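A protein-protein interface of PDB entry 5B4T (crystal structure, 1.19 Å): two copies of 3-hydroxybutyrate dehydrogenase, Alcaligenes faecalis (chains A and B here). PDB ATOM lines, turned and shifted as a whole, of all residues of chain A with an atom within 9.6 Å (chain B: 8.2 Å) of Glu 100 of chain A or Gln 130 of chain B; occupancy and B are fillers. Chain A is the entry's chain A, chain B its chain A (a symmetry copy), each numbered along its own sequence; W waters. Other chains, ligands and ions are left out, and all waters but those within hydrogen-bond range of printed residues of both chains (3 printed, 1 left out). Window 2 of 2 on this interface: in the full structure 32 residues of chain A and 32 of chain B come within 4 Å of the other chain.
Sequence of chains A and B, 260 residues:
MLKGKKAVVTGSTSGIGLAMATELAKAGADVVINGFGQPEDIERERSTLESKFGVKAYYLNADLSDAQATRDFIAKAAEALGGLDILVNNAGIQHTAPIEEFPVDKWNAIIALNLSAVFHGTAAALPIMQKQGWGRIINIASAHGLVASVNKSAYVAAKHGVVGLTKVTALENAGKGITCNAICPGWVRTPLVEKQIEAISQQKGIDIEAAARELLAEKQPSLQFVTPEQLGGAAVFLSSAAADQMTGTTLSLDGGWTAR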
ATOM      1  N   ALA A  97      11.260 -11.882  -3.466  1.00  0.00           N
ATOM      2  CA  ALA A  97      10.685 -10.563  -3.777  1.00  0.00           C
ATOM      3  C   ALA A  97      11.192  -9.615  -2.705  1.00  0.00           C
ATOM      4  O   ALA A  97      11.375 -10.053  -1.575  1.00  0.00           O
ATOM      5  CB  ALA A  97       9.182 -10.621  -3.724  1.00  0.00           C
ATOM      6  N   PRO A  98      11.256  -8.301  -2.989  1.00  0.00           N
ATOM      7  CA  PRO A  98      11.600  -7.445  -1.864  1.00  0.00           C
ATOM      8  C   PRO A  98      10.440  -7.290  -0.889  1.00  0.00           C
ATOM      9  O   PRO A  98       9.294  -7.600  -1.214  1.00  0.00           O
ATOM     10  CB  PRO A  98      11.923  -6.121  -2.534  1.00  0.00           C
ATOM     11  CG  PRO A  98      11.024  -6.105  -3.721  1.00  0.00           C
ATOM     12  CD  PRO A  98      10.897  -7.524  -4.187  1.00  0.00           C
ATOM     13  N   ILE A  99      10.768  -6.903   0.337  1.00  0.00           N
ATOM     14  CA  ILE A  99       9.791  -6.939   1.428  1.00  0.00           C
ATOM     15  C   ILE A  99       8.504  -6.222   1.054  1.00  0.00           C
ATOM     16  O   ILE A  99       7.426  -6.736   1.326  1.00  0.00           O
ATOM     17  CB  ILE A  99      10.400  -6.350   2.723  1.00  0.00           C
ATOM     18  CG1 ILE A  99      11.460  -7.304   3.279  1.00  0.00           C
ATOM     19  CG2 ILE A  99       9.337  -6.116   3.771  1.00  0.00           C
ATOM     20  CD1 ILE A  99      12.429  -6.664   4.257  1.00  0.00           C
ATOM     21  N   GLU A 100       8.620  -5.000   0.562  1.00  0.00           N
ATOM     22  CA  GLU A 100       7.435  -4.188   0.292  1.00  0.00           C
ATOM     23  C   GLU A 100       6.555  -4.716  -0.838  1.00  0.00           C
ATOM     24  O   GLU A 100       5.397  -4.299  -0.938  1.00  0.00           O
ATOM     25  CB  GLU A 100       7.797  -2.727   0.040  1.00  0.00           C
ATOM     26  CG  GLU A 100       8.621  -2.479  -1.206  1.00  0.00           C
ATOM     27  CD  GLU A 100      10.121  -2.664  -1.022  1.00  0.00           C
ATOM     28  OE1 GLU A 100      10.571  -3.260  -0.021  1.00  0.00           O
ATOM     29  OE2 GLU A 100      10.880  -2.241  -1.919  1.00  0.00           O
ATOM     30  N   GLU A 101       7.035  -5.704  -1.583  1.00  0.00           N
ATOM     31  CA  GLU A 101       6.282  -6.385  -2.634  1.00  0.00           C
ATOM     32  C   GLU A 101       5.993  -7.849  -2.283  1.00  0.00           C
ATOM     33  O   GLU A 101       5.547  -8.616  -3.147  1.00  0.00           O
ATOM     34  CB  GLU A 101       7.075  -6.367  -3.957  1.00  0.00           C
ATOM     35  CG  GLU A 101       7.428  -4.983  -4.471  1.00  0.00           C
ATOM     36  CD  GLU A 101       8.386  -5.037  -5.652  1.00  0.00           C
ATOM     37  OE1 GLU A 101       8.564  -6.135  -6.224  1.00  0.00           O
ATOM     38  OE2 GLU A 101       9.076  -4.026  -5.897  1.00  0.00           O
ATOM     39  N   PHE A 102       6.419  -8.304  -1.116  1.00  0.00           N
ATOM     40  CA  PHE A 102       6.434  -9.721  -0.831  1.00  0.00           C
ATOM     41  C   PHE A 102       5.016 -10.159  -0.534  1.00  0.00           C
ATOM     42  O   PHE A 102       4.376  -9.591   0.331  1.00  0.00           O
ATOM     43  CB  PHE A 102       7.305 -10.013   0.386  1.00  0.00           C
ATOM     44  CG  PHE A 102       7.774 -11.433   0.464  1.00  0.00           C
ATOM     45  CD1 PHE A 102       9.032 -11.768   0.010  1.00  0.00           C
ATOM     46  CD2 PHE A 102       6.939 -12.451   0.906  1.00  0.00           C
ATOM     47  CE1 PHE A 102       9.454 -13.067   0.013  1.00  0.00           C
ATOM     48  CE2 PHE A 102       7.381 -13.755   0.939  1.00  0.00           C
ATOM     49  CZ  PHE A 102       8.615 -14.060   0.457  1.00  0.00           C
ATOM     50  N   PRO A 103       4.453 -11.101  -1.300  1.00  0.00           N
ATOM     51  CA  PRO A 103       3.043 -11.412  -1.101  1.00  0.00           C
ATOM     52  C   PRO A 103       2.758 -11.895   0.316  1.00  0.00           C
ATOM     53  O   PRO A 103       3.433 -12.787   0.812  1.00  0.00           O
ATOM     54  CB  PRO A 103       2.787 -12.513  -2.143  1.00  0.00           C
ATOM     55  CG  PRO A 103       3.807 -12.254  -3.197  1.00  0.00           C
ATOM     56  CD  PRO A 103       5.023 -11.800  -2.463  1.00  0.00           C
ATOM     57  N   VAL A 104       1.699 -11.384   0.922  1.00  0.00           N
ATOM     58  CA  VAL A 104       1.305 -11.798   2.246  1.00  0.00           C
ATOM     59  C   VAL A 104       1.036 -13.305   2.301  1.00  0.00           C
ATOM     60  O   VAL A 104       1.418 -14.008   3.265  1.00  0.00           O
ATOM     61  CB  VAL A 104       0.103 -10.965   2.726  1.00  0.00           C
ATOM     62  CG1 VAL A 104      -0.546 -11.621   3.926  1.00  0.00           C
ATOM     63  CG2 VAL A 104       0.522  -9.530   3.028  1.00  0.00           C
ATOM     64  N   ASN A 151      15.780 -10.088  -0.683  1.00  0.00           N
ATOM     65  CA  ASN A 151      14.602 -10.600  -1.352  1.00  0.00           C
ATOM     66  C   ASN A 151      14.130 -11.936  -0.833  1.00  0.00           C
ATOM     67  O   ASN A 151      13.287 -12.568  -1.441  1.00  0.00           O
ATOM     68  CB  ASN A 151      14.754 -10.592  -2.866  1.00  0.00           C
ATOM     69  CG  ASN A 151      14.985  -9.197  -3.413  1.00  0.00           C
ATOM     70  OD1 ASN A 151      14.692  -8.206  -2.774  1.00  0.00           O
ATOM     71  ND2 ASN A 151      15.715  -9.134  -4.523  1.00  0.00           N
ATOM     72  N   LYS A 152      14.602 -12.294   0.360  1.00  0.00           N
ATOM     73  CA  LYS A 152      14.258 -13.577   0.943  1.00  0.00           C
ATOM     74  C   LYS A 152      13.754 -13.397   2.364  1.00  0.00           C
ATOM     75  O   LYS A 152      14.030 -14.214   3.235  1.00  0.00           O
ATOM     76  CB  LYS A 152      15.440 -14.538   0.875  1.00  0.00           C
ATOM     77  CG  LYS A 152      15.687 -15.004  -0.550  1.00  0.00           C
ATOM     78  CD  LYS A 152      16.861 -15.944  -0.688  1.00  0.00           C
ATOM     79  CE  LYS A 152      16.948 -16.450  -2.106  1.00  0.00           C
ATOM     80  NZ  LYS A 152      18.088 -17.384  -2.277  1.00  0.00           N
ATOM     81  N   SER A 153      12.992 -12.333   2.628  1.00  0.00           N
ATOM     82  CA  SER A 153      12.545 -12.050   3.997  1.00  0.00           C
ATOM     83  C   SER A 153      11.873 -13.237   4.663  1.00  0.00           C
ATOM     84  O   SER A 153      12.256 -13.610   5.787  1.00  0.00           O
ATOM     85  CB  SER A 153      11.622 -10.857   4.040  1.00  0.00           C
ATOM     86  OG  SER A 153      10.541 -10.991   3.148  1.00  0.00           O
ATOM     87  N   ARG B  71      -0.872  -3.384   8.561  1.00  0.00           N
ATOM     88  CA  ARG B  71      -0.614  -2.559   7.405  1.00  0.00           C
ATOM     89  C   ARG B  71      -1.471  -1.278   7.430  1.00  0.00           C
ATOM     90  O   ARG B  71      -0.960  -0.192   7.171  1.00  0.00           O
ATOM     91  CB  ARG B  71      -0.805  -3.361   6.116  1.00  0.00           C
ATOM     92  CG  ARG B  71       0.291  -4.412   5.986  1.00  0.00           C
ATOM     93  CD  ARG B  71      -0.009  -5.456   4.937  1.00  0.00           C
ATOM     94  NE  ARG B  71       1.084  -6.418   4.821  1.00  0.00           N
ATOM     95  CZ  ARG B  71       2.078  -6.365   3.940  1.00  0.00           C
ATOM     96  NH1 ARG B  71       2.082  -5.485   2.954  1.00  0.00           N
ATOM     97  NH2 ARG B  71       3.061  -7.229   4.037  1.00  0.00           N
ATOM     98  N   LEU B  84       6.718   9.325   8.286  1.00  0.00           N
ATOM     99  CA  LEU B  84       7.147   8.226   9.153  1.00  0.00           C
ATOM    100  C   LEU B  84       8.648   8.034   9.008  1.00  0.00           C
ATOM    101  O   LEU B  84       9.119   7.600   7.946  1.00  0.00           O
ATOM    102  CB  LEU B  84       6.400   6.930   8.805  1.00  0.00           C
ATOM    103  CG  LEU B  84       6.146   5.938   9.961  1.00  0.00           C
ATOM    104  CD1 LEU B  84       5.257   4.789   9.516  1.00  0.00           C
ATOM    105  CD2 LEU B  84       7.436   5.394  10.534  1.00  0.00           C
ATOM    106  N   PHE B 119       7.257  -8.046  10.053  1.00  0.00           N
ATOM    107  CA  PHE B 119       7.228  -8.072   8.610  1.00  0.00           C
ATOM    108  C   PHE B 119       6.176  -7.123   8.047  1.00  0.00           C
ATOM    109  O   PHE B 119       6.485  -6.290   7.188  1.00  0.00           O
ATOM    110  CB  PHE B 119       6.982  -9.493   8.104  1.00  0.00           C
ATOM    111  CG  PHE B 119       6.604  -9.550   6.667  1.00  0.00           C
ATOM    112  CD1 PHE B 119       7.570  -9.421   5.663  1.00  0.00           C
ATOM    113  CD2 PHE B 119       5.322  -9.885   6.299  1.00  0.00           C
ATOM    114  CE1 PHE B 119       7.174  -9.430   4.340  1.00  0.00           C
ATOM    115  CE2 PHE B 119       4.965 -10.000   4.957  1.00  0.00           C
ATOM    116  CZ  PHE B 119       5.914  -9.823   4.004  1.00  0.00           C
ATOM    117  N   HIS B 120       4.938  -7.241   8.519  1.00  0.00           N
ATOM    118  CA  HIS B 120       3.882  -6.429   7.919  1.00  0.00           C
ATOM    119  C   HIS B 120       4.083  -4.946   8.204  1.00  0.00           C
ATOM    120  O   HIS B 120       3.873  -4.095   7.315  1.00  0.00           O
ATOM    121  CB  HIS B 120       2.521  -6.856   8.438  1.00  0.00           C
ATOM    122  CG  HIS B 120       2.159  -8.231   8.025  1.00  0.00           C
ATOM    123  ND1 HIS B 120       2.063  -8.613   6.699  1.00  0.00           N
ATOM    124  CD2 HIS B 120       1.928  -9.338   8.758  1.00  0.00           C
ATOM    125  CE1 HIS B 120       1.826  -9.908   6.645  1.00  0.00           C
ATOM    126  NE2 HIS B 120       1.722 -10.368   7.877  1.00  0.00           N
ATOM    127  N   THR B 122       7.004  -3.403   8.726  1.00  0.00           N
ATOM    128  CA  THR B 122       8.133  -2.997   7.908  1.00  0.00           C
ATOM    129  C   THR B 122       7.690  -2.787   6.466  1.00  0.00           C
ATOM    130  O   THR B 122       8.123  -1.848   5.810  1.00  0.00           O
ATOM    131  CB  THR B 122       9.235  -4.054   8.030  1.00  0.00           C
ATOM    132  OG1 THR B 122       9.728  -4.095   9.384  1.00  0.00           O
ATOM    133  CG2 THR B 122      10.391  -3.741   7.108  1.00  0.00           C
ATOM    134  N   ALA B 123       6.965  -3.752   5.929  1.00  0.00           N
ATOM    135  CA  ALA B 123       6.514  -3.686   4.548  1.00  0.00           C
ATOM    136  C   ALA B 123       5.724  -2.431   4.271  1.00  0.00           C
ATOM    137  O   ALA B 123       5.872  -1.798   3.218  1.00  0.00           O
ATOM    138  CB  ALA B 123       5.680  -4.901   4.214  1.00  0.00           C
ATOM    139  N   ALA B 124       4.879  -2.058   5.216  1.00  0.00           N
ATOM    140  CA  ALA B 124       4.061  -0.843   5.082  1.00  0.00           C
ATOM    141  C   ALA B 124       4.910   0.418   5.224  1.00  0.00           C
ATOM    142  O   ALA B 124       4.603   1.446   4.609  1.00  0.00           O
ATOM    143  CB  ALA B 124       2.902  -0.855   6.076  1.00  0.00           C
ATOM    144  N   ALA B 125       5.895   0.411   6.104  1.00  0.00           N
ATOM    145  CA  ALA B 125       6.666   1.616   6.382  1.00  0.00           C
ATOM    146  C   ALA B 125       7.674   1.912   5.296  1.00  0.00           C
ATOM    147  O   ALA B 125       8.033   3.059   5.067  1.00  0.00           O
ATOM    148  CB  ALA B 125       7.353   1.507   7.735  1.00  0.00           C
ATOM    149  N   LEU B 126       8.254   0.864   4.722  1.00  0.00           N
ATOM    150  CA  LEU B 126       9.413   1.036   3.851  1.00  0.00           C
ATOM    151  C   LEU B 126       9.170   1.989   2.711  1.00  0.00           C
ATOM    152  O   LEU B 126      10.044   2.784   2.434  1.00  0.00           O
ATOM    153  CB  LEU B 126       9.947  -0.295   3.325  1.00  0.00           C
ATOM    154  CG  LEU B 126      10.879  -1.026   4.296  1.00  0.00           C
ATOM    155  CD1 LEU B 126      11.186  -2.439   3.825  1.00  0.00           C
ATOM    156  CD2 LEU B 126      12.159  -0.232   4.491  1.00  0.00           C
ATOM    157  N   PRO B 127       8.020   1.933   2.019  1.00  0.00           N
ATOM    158  CA  PRO B 127       7.914   2.819   0.842  1.00  0.00           C
ATOM    159  C   PRO B 127       7.931   4.297   1.201  1.00  0.00           C
ATOM    160  O   PRO B 127       8.491   5.108   0.478  1.00  0.00           O
ATOM    161  CB  PRO B 127       6.582   2.419   0.203  1.00  0.00           C
ATOM    162  CG  PRO B 127       6.420   0.995   0.618  1.00  0.00           C
ATOM    163  CD  PRO B 127       6.973   0.903   2.016  1.00  0.00           C
ATOM    164  N   ILE B 128       7.434   4.593   2.394  1.00  0.00           N
ATOM    165  CA  ILE B 128       7.453   5.958   2.909  1.00  0.00           C
ATOM    166  C   ILE B 128       8.899   6.402   3.122  1.00  0.00           C
ATOM    167  O   ILE B 128       9.342   7.487   2.728  1.00  0.00           O
ATOM    168  CB  ILE B 128       6.623   6.032   4.200  1.00  0.00           C
ATOM    169  CG1 ILE B 128       5.190   5.622   3.895  1.00  0.00           C
ATOM    170  CG2 ILE B 128       6.653   7.432   4.777  1.00  0.00           C
ATOM    171  CD1 ILE B 128       4.338   5.407   5.129  1.00  0.00           C
ATOM    172  N   MET B 129       9.674   5.550   3.793  1.00  0.00           N
ATOM    173  CA  MET B 129      11.061   5.848   4.076  1.00  0.00           C
ATOM    174  C   MET B 129      11.893   5.878   2.809  1.00  0.00           C
ATOM    175  O   MET B 129      12.803   6.682   2.679  1.00  0.00           O
ATOM    176  CB  MET B 129      11.625   4.818   5.033  1.00  0.00           C
ATOM    177  CG  MET B 129      10.950   4.832   6.369  1.00  0.00           C
ATOM    178  SD  MET B 129      11.589   3.517   7.423  1.00  0.00           S
ATOM    179  CE  MET B 129      10.724   3.905   8.954  1.00  0.00           C
ATOM    180  N   GLN B 130      11.603   5.000   1.866  1.00  0.00           N
ATOM    181  CA  GLN B 130      12.360   4.951   0.600  1.00  0.00           C
ATOM    182  C   GLN B 130      12.184   6.237  -0.195  1.00  0.00           C
ATOM    183  O   GLN B 130      13.148   6.789  -0.716  1.00  0.00           O
ATOM    184  CB  GLN B 130      11.931   3.737  -0.207  1.00  0.00           C
ATOM    185  CG  GLN B 130      12.460   2.447   0.410  1.00  0.00           C
ATOM    186  CD  GLN B 130      11.809   1.185  -0.123  1.00  0.00           C
ATOM    187  OE1 GLN B 130      12.297   0.076   0.114  1.00  0.00           O
ATOM    188  NE2 GLN B 130      10.672   1.325  -0.772  1.00  0.00           N
ATOM    189  N   LYS B 131      10.997   6.813  -0.147  1.00  0.00           N
ATOM    190  CA  LYS B 131      10.703   8.028  -0.924  1.00  0.00           C
ATOM    191  C   LYS B 131      11.348   9.259  -0.335  1.00  0.00           C
ATOM    192  O   LYS B 131      11.784  10.142  -1.070  1.00  0.00           O
ATOM    193  CB  LYS B 131       9.203   8.233  -1.053  1.00  0.00           C
ATOM    194  CG  LYS B 131       8.583   7.227  -2.006  1.00  0.00           C
ATOM    195  CD  LYS B 131       7.355   7.786  -2.707  1.00  0.00           C
ATOM    196  CE  LYS B 131       6.630   6.702  -3.494  1.00  0.00           C
ATOM    197  NZ  LYS B 131       6.304   5.510  -2.658  1.00  0.00           N
ATOM    198  N   GLN B 132      11.626   9.237   0.956  1.00  0.00           N
ATOM    199  CA  GLN B 132      12.278  10.374   1.575  1.00  0.00           C
ATOM    200  C   GLN B 132      13.769  10.180   1.790  1.00  0.00           C
ATOM    201  O   GLN B 132      14.487  11.133   2.042  1.00  0.00           O
ATOM    202  CB  GLN B 132      11.623  10.671   2.891  1.00  0.00           C
ATOM    203  CG  GLN B 132      11.917   9.631   3.940  1.00  0.00           C
ATOM    204  CD  GLN B 132      10.868   9.601   5.030  1.00  0.00           C
ATOM    205  OE1 GLN B 132      11.026   8.934   6.062  1.00  0.00           O
ATOM    206  NE2 GLN B 132       9.764  10.287   4.785  1.00  0.00           N
ATOM    207  N   GLY B 133      14.264   8.992   1.489  1.00  0.00           N
ATOM    208  CA  GLY B 133      15.681   8.707   1.594  1.00  0.00           C
ATOM    209  C   GLY B 133      16.235   8.756   3.005  1.00  0.00           C
ATOM    210  O   GLY B 133      17.391   8.996   3.198  1.00  0.00           O
ATOM    211  N   TRP B 134      15.408   8.451   3.996  1.00  0.00           N
ATOM    212  CA  TRP B 134      15.873   8.373   5.393  1.00  0.00           C
ATOM    213  C   TRP B 134      14.887   7.519   6.164  1.00  0.00           C
ATOM    214  O   TRP B 134      13.677   7.656   5.984  1.00  0.00           O
ATOM    215  CB  TRP B 134      15.973   9.758   6.057  1.00  0.00           C
ATOM    216  CG  TRP B 134      16.813   9.770   7.301  1.00  0.00           C
ATOM    217  CD1 TRP B 134      18.156  10.021   7.354  1.00  0.00           C
ATOM    218  CD2 TRP B 134      16.400   9.517   8.655  1.00  0.00           C
ATOM    219  NE1 TRP B 134      18.598   9.950   8.639  1.00  0.00           N
ATOM    220  CE2 TRP B 134      17.549   9.623   9.459  1.00  0.00           C
ATOM    221  CE3 TRP B 134      15.191   9.143   9.260  1.00  0.00           C
ATOM    222  CZ2 TRP B 134      17.531   9.350  10.818  1.00  0.00           C
ATOM    223  CZ3 TRP B 134      15.189   8.897  10.603  1.00  0.00           C
ATOM    224  CH2 TRP B 134      16.331   9.048  11.380  1.00  0.00           C
ATOM    225  N   GLY B 135      15.389   6.654   7.032  1.00  0.00           N
ATOM    226  CA  GLY B 135      14.508   5.907   7.891  1.00  0.00           C
ATOM    227  C   GLY B 135      15.293   5.136   8.912  1.00  0.00           C
ATOM    228  O   GLY B 135      16.489   4.830   8.726  1.00  0.00           O
ATOM    229  N   THR B 169      16.008  -6.790   5.841  1.00  0.00           N
ATOM    230  CA  THR B 169      15.547  -5.434   5.674  1.00  0.00           C
ATOM    231  C   THR B 169      16.741  -4.509   5.426  1.00  0.00           C
ATOM    232  O   THR B 169      16.710  -3.616   4.565  1.00  0.00           O
ATOM    233  CB  THR B 169      14.759  -4.991   6.932  1.00  0.00           C
ATOM    234  OG1 THR B 169      13.689  -5.884   7.181  1.00  0.00           O
ATOM    235  CG2 THR B 169      14.204  -3.588   6.774  1.00  0.00           C
ATOM    236  N   GLU B 172      18.307  -5.091   1.906  1.00  0.00           N
ATOM    237  CA  GLU B 172      17.465  -4.602   0.800  1.00  0.00           C
ATOM    238  C   GLU B 172      17.511  -3.093   0.697  1.00  0.00           C
ATOM    239  O   GLU B 172      17.194  -2.531  -0.364  1.00  0.00           O
ATOM    240  CB  GLU B 172      16.037  -5.073   0.982  1.00  0.00           C
ATOM    241  CG  GLU B 172      15.864  -6.562   0.724  1.00  0.00           C
ATOM    242  CD  GLU B 172      14.409  -7.031   0.807  1.00  0.00           C
ATOM    243  OE1 GLU B 172      13.466  -6.194   0.906  1.00  0.00           O
ATOM    244  OE2 GLU B 172      14.191  -8.256   0.741  1.00  0.00           O
ATOM    245  N   ASN B 173      17.815  -2.426   1.797  1.00  0.00           N
ATOM    246  CA  ASN B 173      17.748  -0.975   1.841  1.00  0.00           C
ATOM    247  C   ASN B 173      19.101  -0.348   2.088  1.00  0.00           C
ATOM    248  O   ASN B 173      19.236   0.855   2.320  1.00  0.00           O
ATOM    249  CB  ASN B 173      16.722  -0.548   2.861  1.00  0.00           C
ATOM    250  CG  ASN B 173      15.334  -0.980   2.459  1.00  0.00           C
ATOM    251  OD1 ASN B 173      14.844  -2.048   2.861  1.00  0.00           O
ATOM    252  ND2 ASN B 173      14.766  -0.284   1.513  1.00  0.00           N
ATOM    253  N   ALA B 174      20.141  -1.131   1.841  1.00  0.00           N
ATOM    254  CA  ALA B 174      21.502  -0.687   2.084  1.00  0.00           C
ATOM    255  C   ALA B 174      21.830   0.508   1.200  1.00  0.00           C
ATOM    256  O   ALA B 174      21.600   0.469  -0.002  1.00  0.00           O
ATOM    257  CB  ALA B 174      22.472  -1.819   1.819  1.00  0.00           C
ATOM    258  N   LYS B 176      20.406   3.353   1.165  1.00  0.00           N
ATOM    259  CA  LYS B 176      19.257   4.192   0.824  1.00  0.00           C
ATOM    260  C   LYS B 176      19.000   5.269   1.869  1.00  0.00           C
ATOM    261  O   LYS B 176      18.003   6.006   1.743  1.00  0.00           O
ATOM    262  CB  LYS B 176      17.989   3.366   0.654  1.00  0.00           C
ATOM    263  CG  LYS B 176      17.994   2.442  -0.532  1.00  0.00           C
ATOM    264  CD  LYS B 176      16.656   1.754  -0.676  1.00  0.00           C
ATOM    265  CE  LYS B 176      16.700   0.657  -1.726  1.00  0.00           C
ATOM    266  NZ  LYS B 176      15.454  -0.151  -1.666  1.00  0.00           N
ATOM    267  N   GLY B 177      19.736   5.267   2.965  1.00  0.00           N
ATOM    268  CA  GLY B 177      19.477   6.201   4.058  1.00  0.00           C
ATOM    269  C   GLY B 177      18.595   5.576   5.137  1.00  0.00           C
ATOM    270  O   GLY B 177      18.249   6.221   6.124  1.00  0.00           O
ATOM    271  N   ILE B 178      18.286   4.304   4.957  1.00  0.00           N
ATOM    272  CA  ILE B 178      17.437   3.571   5.889  1.00  0.00           C
ATOM    273  C   ILE B 178      18.246   2.465   6.527  1.00  0.00           C
ATOM    274  O   ILE B 178      18.922   1.689   5.816  1.00  0.00           O
ATOM    275  CB  ILE B 178      16.308   2.885   5.114  1.00  0.00           C
ATOM    276  CG1 ILE B 178      15.466   3.928   4.380  1.00  0.00           C
ATOM    277  CG2 ILE B 178      15.417   2.089   6.049  1.00  0.00           C
ATOM    278  CD1 ILE B 178      14.524   3.324   3.366  1.00  0.00           C
HETATM  279  O   HOH W   1       4.327  -1.784   1.001  1.00  0.00           O
HETATM  280  O   HOH W   2      12.157 -10.029   1.031  1.00  0.00           O
HETATM  281  O   HOH W   3       4.650  -7.244   1.688  1.00  0.00           O
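The side-chain carboxylate (OE2) of Glu 100 of chain A sits close to the side-chain amide oxygen (OE1) of Gln 130 of chain B (3.4 Å).
N of Ile 99 of chain A sits at hydrogen-bond distance from OE1 of Glu 172 of chain B (2.8 Å).
The side-chain carboxylate (OE2) of Glu 172 of chain B sits at hydrogen-bond distance from the backbone NH (N) of Asn 151 of chain A, at 2.8 Å.
The side-chain amino group of Lys 176 of chain B is in hydrogen-bond range of the backbone carbonyl oxygen of Glu 172 of chain B, 3.2 Å away.
The backbone carbonyl oxygen (O) of Asn 151 of chain A sits at hydrogen-bond distance from the backbone NH (N) of Ala 97 of chain A, at 2.9 Å.
The side-chain amide oxygen (OD1) of Asn 173 of chain B sits close to the backbone carbonyl oxygen (O) of Thr 169 of chain B, at 3.0 Å.
NE of Arg 71 of chain B sits at hydrogen-bond distance from ND1 of His 120 of chain B, 3.1 Å away.
OE1 of Gln 130 of chain B is in hydrogen-bond range of ND2 of Asn 173 of chain B.
Among the printed residues, pairs that only touch across the chains: Pro 98 of chain A with Glu 172 of chain B, Ile 99 of chain A with Phe 119 of chain B, Ile 99 of chain A with Ala 123 of chain B, Ile 99 of chain A with Thr 169 of chain B, Glu 100 of chain A with Ala 123 of chain B, Glu 100 of chain A with Leu 126 of chain B, Phe 102 of chain A with Phe 119 of chain B, Val 104 of chain A with Arg 71 of chain B, Val 104 of chain A with His 120 of chain B and Ser 153 of chain A with Phe 119 of chain B.
Of the printed residues of chain B, Glu 100 of chain A touches Ala 123 (3.8 Å), Leu 126 (3.98 Å) and Gln 130 (3.4 Å).
Of chain A, only Glu 100 (3.4 Å) comes within 4 Å of Gln 130 of chain B.
Of the printed residues of chain B, Pro 98 of chain A touches Glu 172 (3.6 Å).
Printed residues of chain A within 4 Å of Glu 172 of chain B: Pro 98, Ile 99 and Asn 151.
Of the printed residues of chain B, Ile 99 of chain A touches Phe 119, Ala 123, Thr 169 and Glu 172.
Glu 101 of chain A touches none of the printed residues of chain B.
Ala 125 of chain B touches none of the printed residues of chain A.
The nearest printed residue of chain B that does not touch Glu 100 of chain A is Pro 127 of chain B (4.01 Å).
Of the 25 printed residues of chain B, 8 touch a printed residue of chain A.
Printed residues of chain B that touch a printed residue of chain A: Arg 71, Phe 119, His 120, Ala 123, Leu 126, Gln 130, Thr 169 and Glu 172.
Hydrophobic or aromatic side chains of chain B that line the printed part of chain A: Phe 119, His 120, Ala 123 and Leu 126.
Along chain B the printed residues that touch a printed residue of chain A span positions 71 to 172.
Hydrophobic or aromatic side chains of chain A that line the printed part of chain B: Pro 98, Ile 99, Phe 102 and Val 104.
No position is printed for both chains.
Water W1 bridges O of Ala 123 of chain B (2.7 Å) and O of Glu 100 of chain A (3.4 Å).
Water W2 lies within hydrogen-bond range of OE2 of Glu 172 of chain B (2.7 Å), O of Ala 97 of chain A (2.7 Å), OG of Ser 153 of chain A (2.8 Å), N of Lys 152 of chain A (3.4 Å) and N of Ile 99 of chain A (3.5 Å).
Water W3 lies within hydrogen-bond range of O of Phe 102 of chain A (2.7 Å), NH2 of Arg 71 of chain B (2.8 Å) and O of Ile 99 of chain A (2.8 Å).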
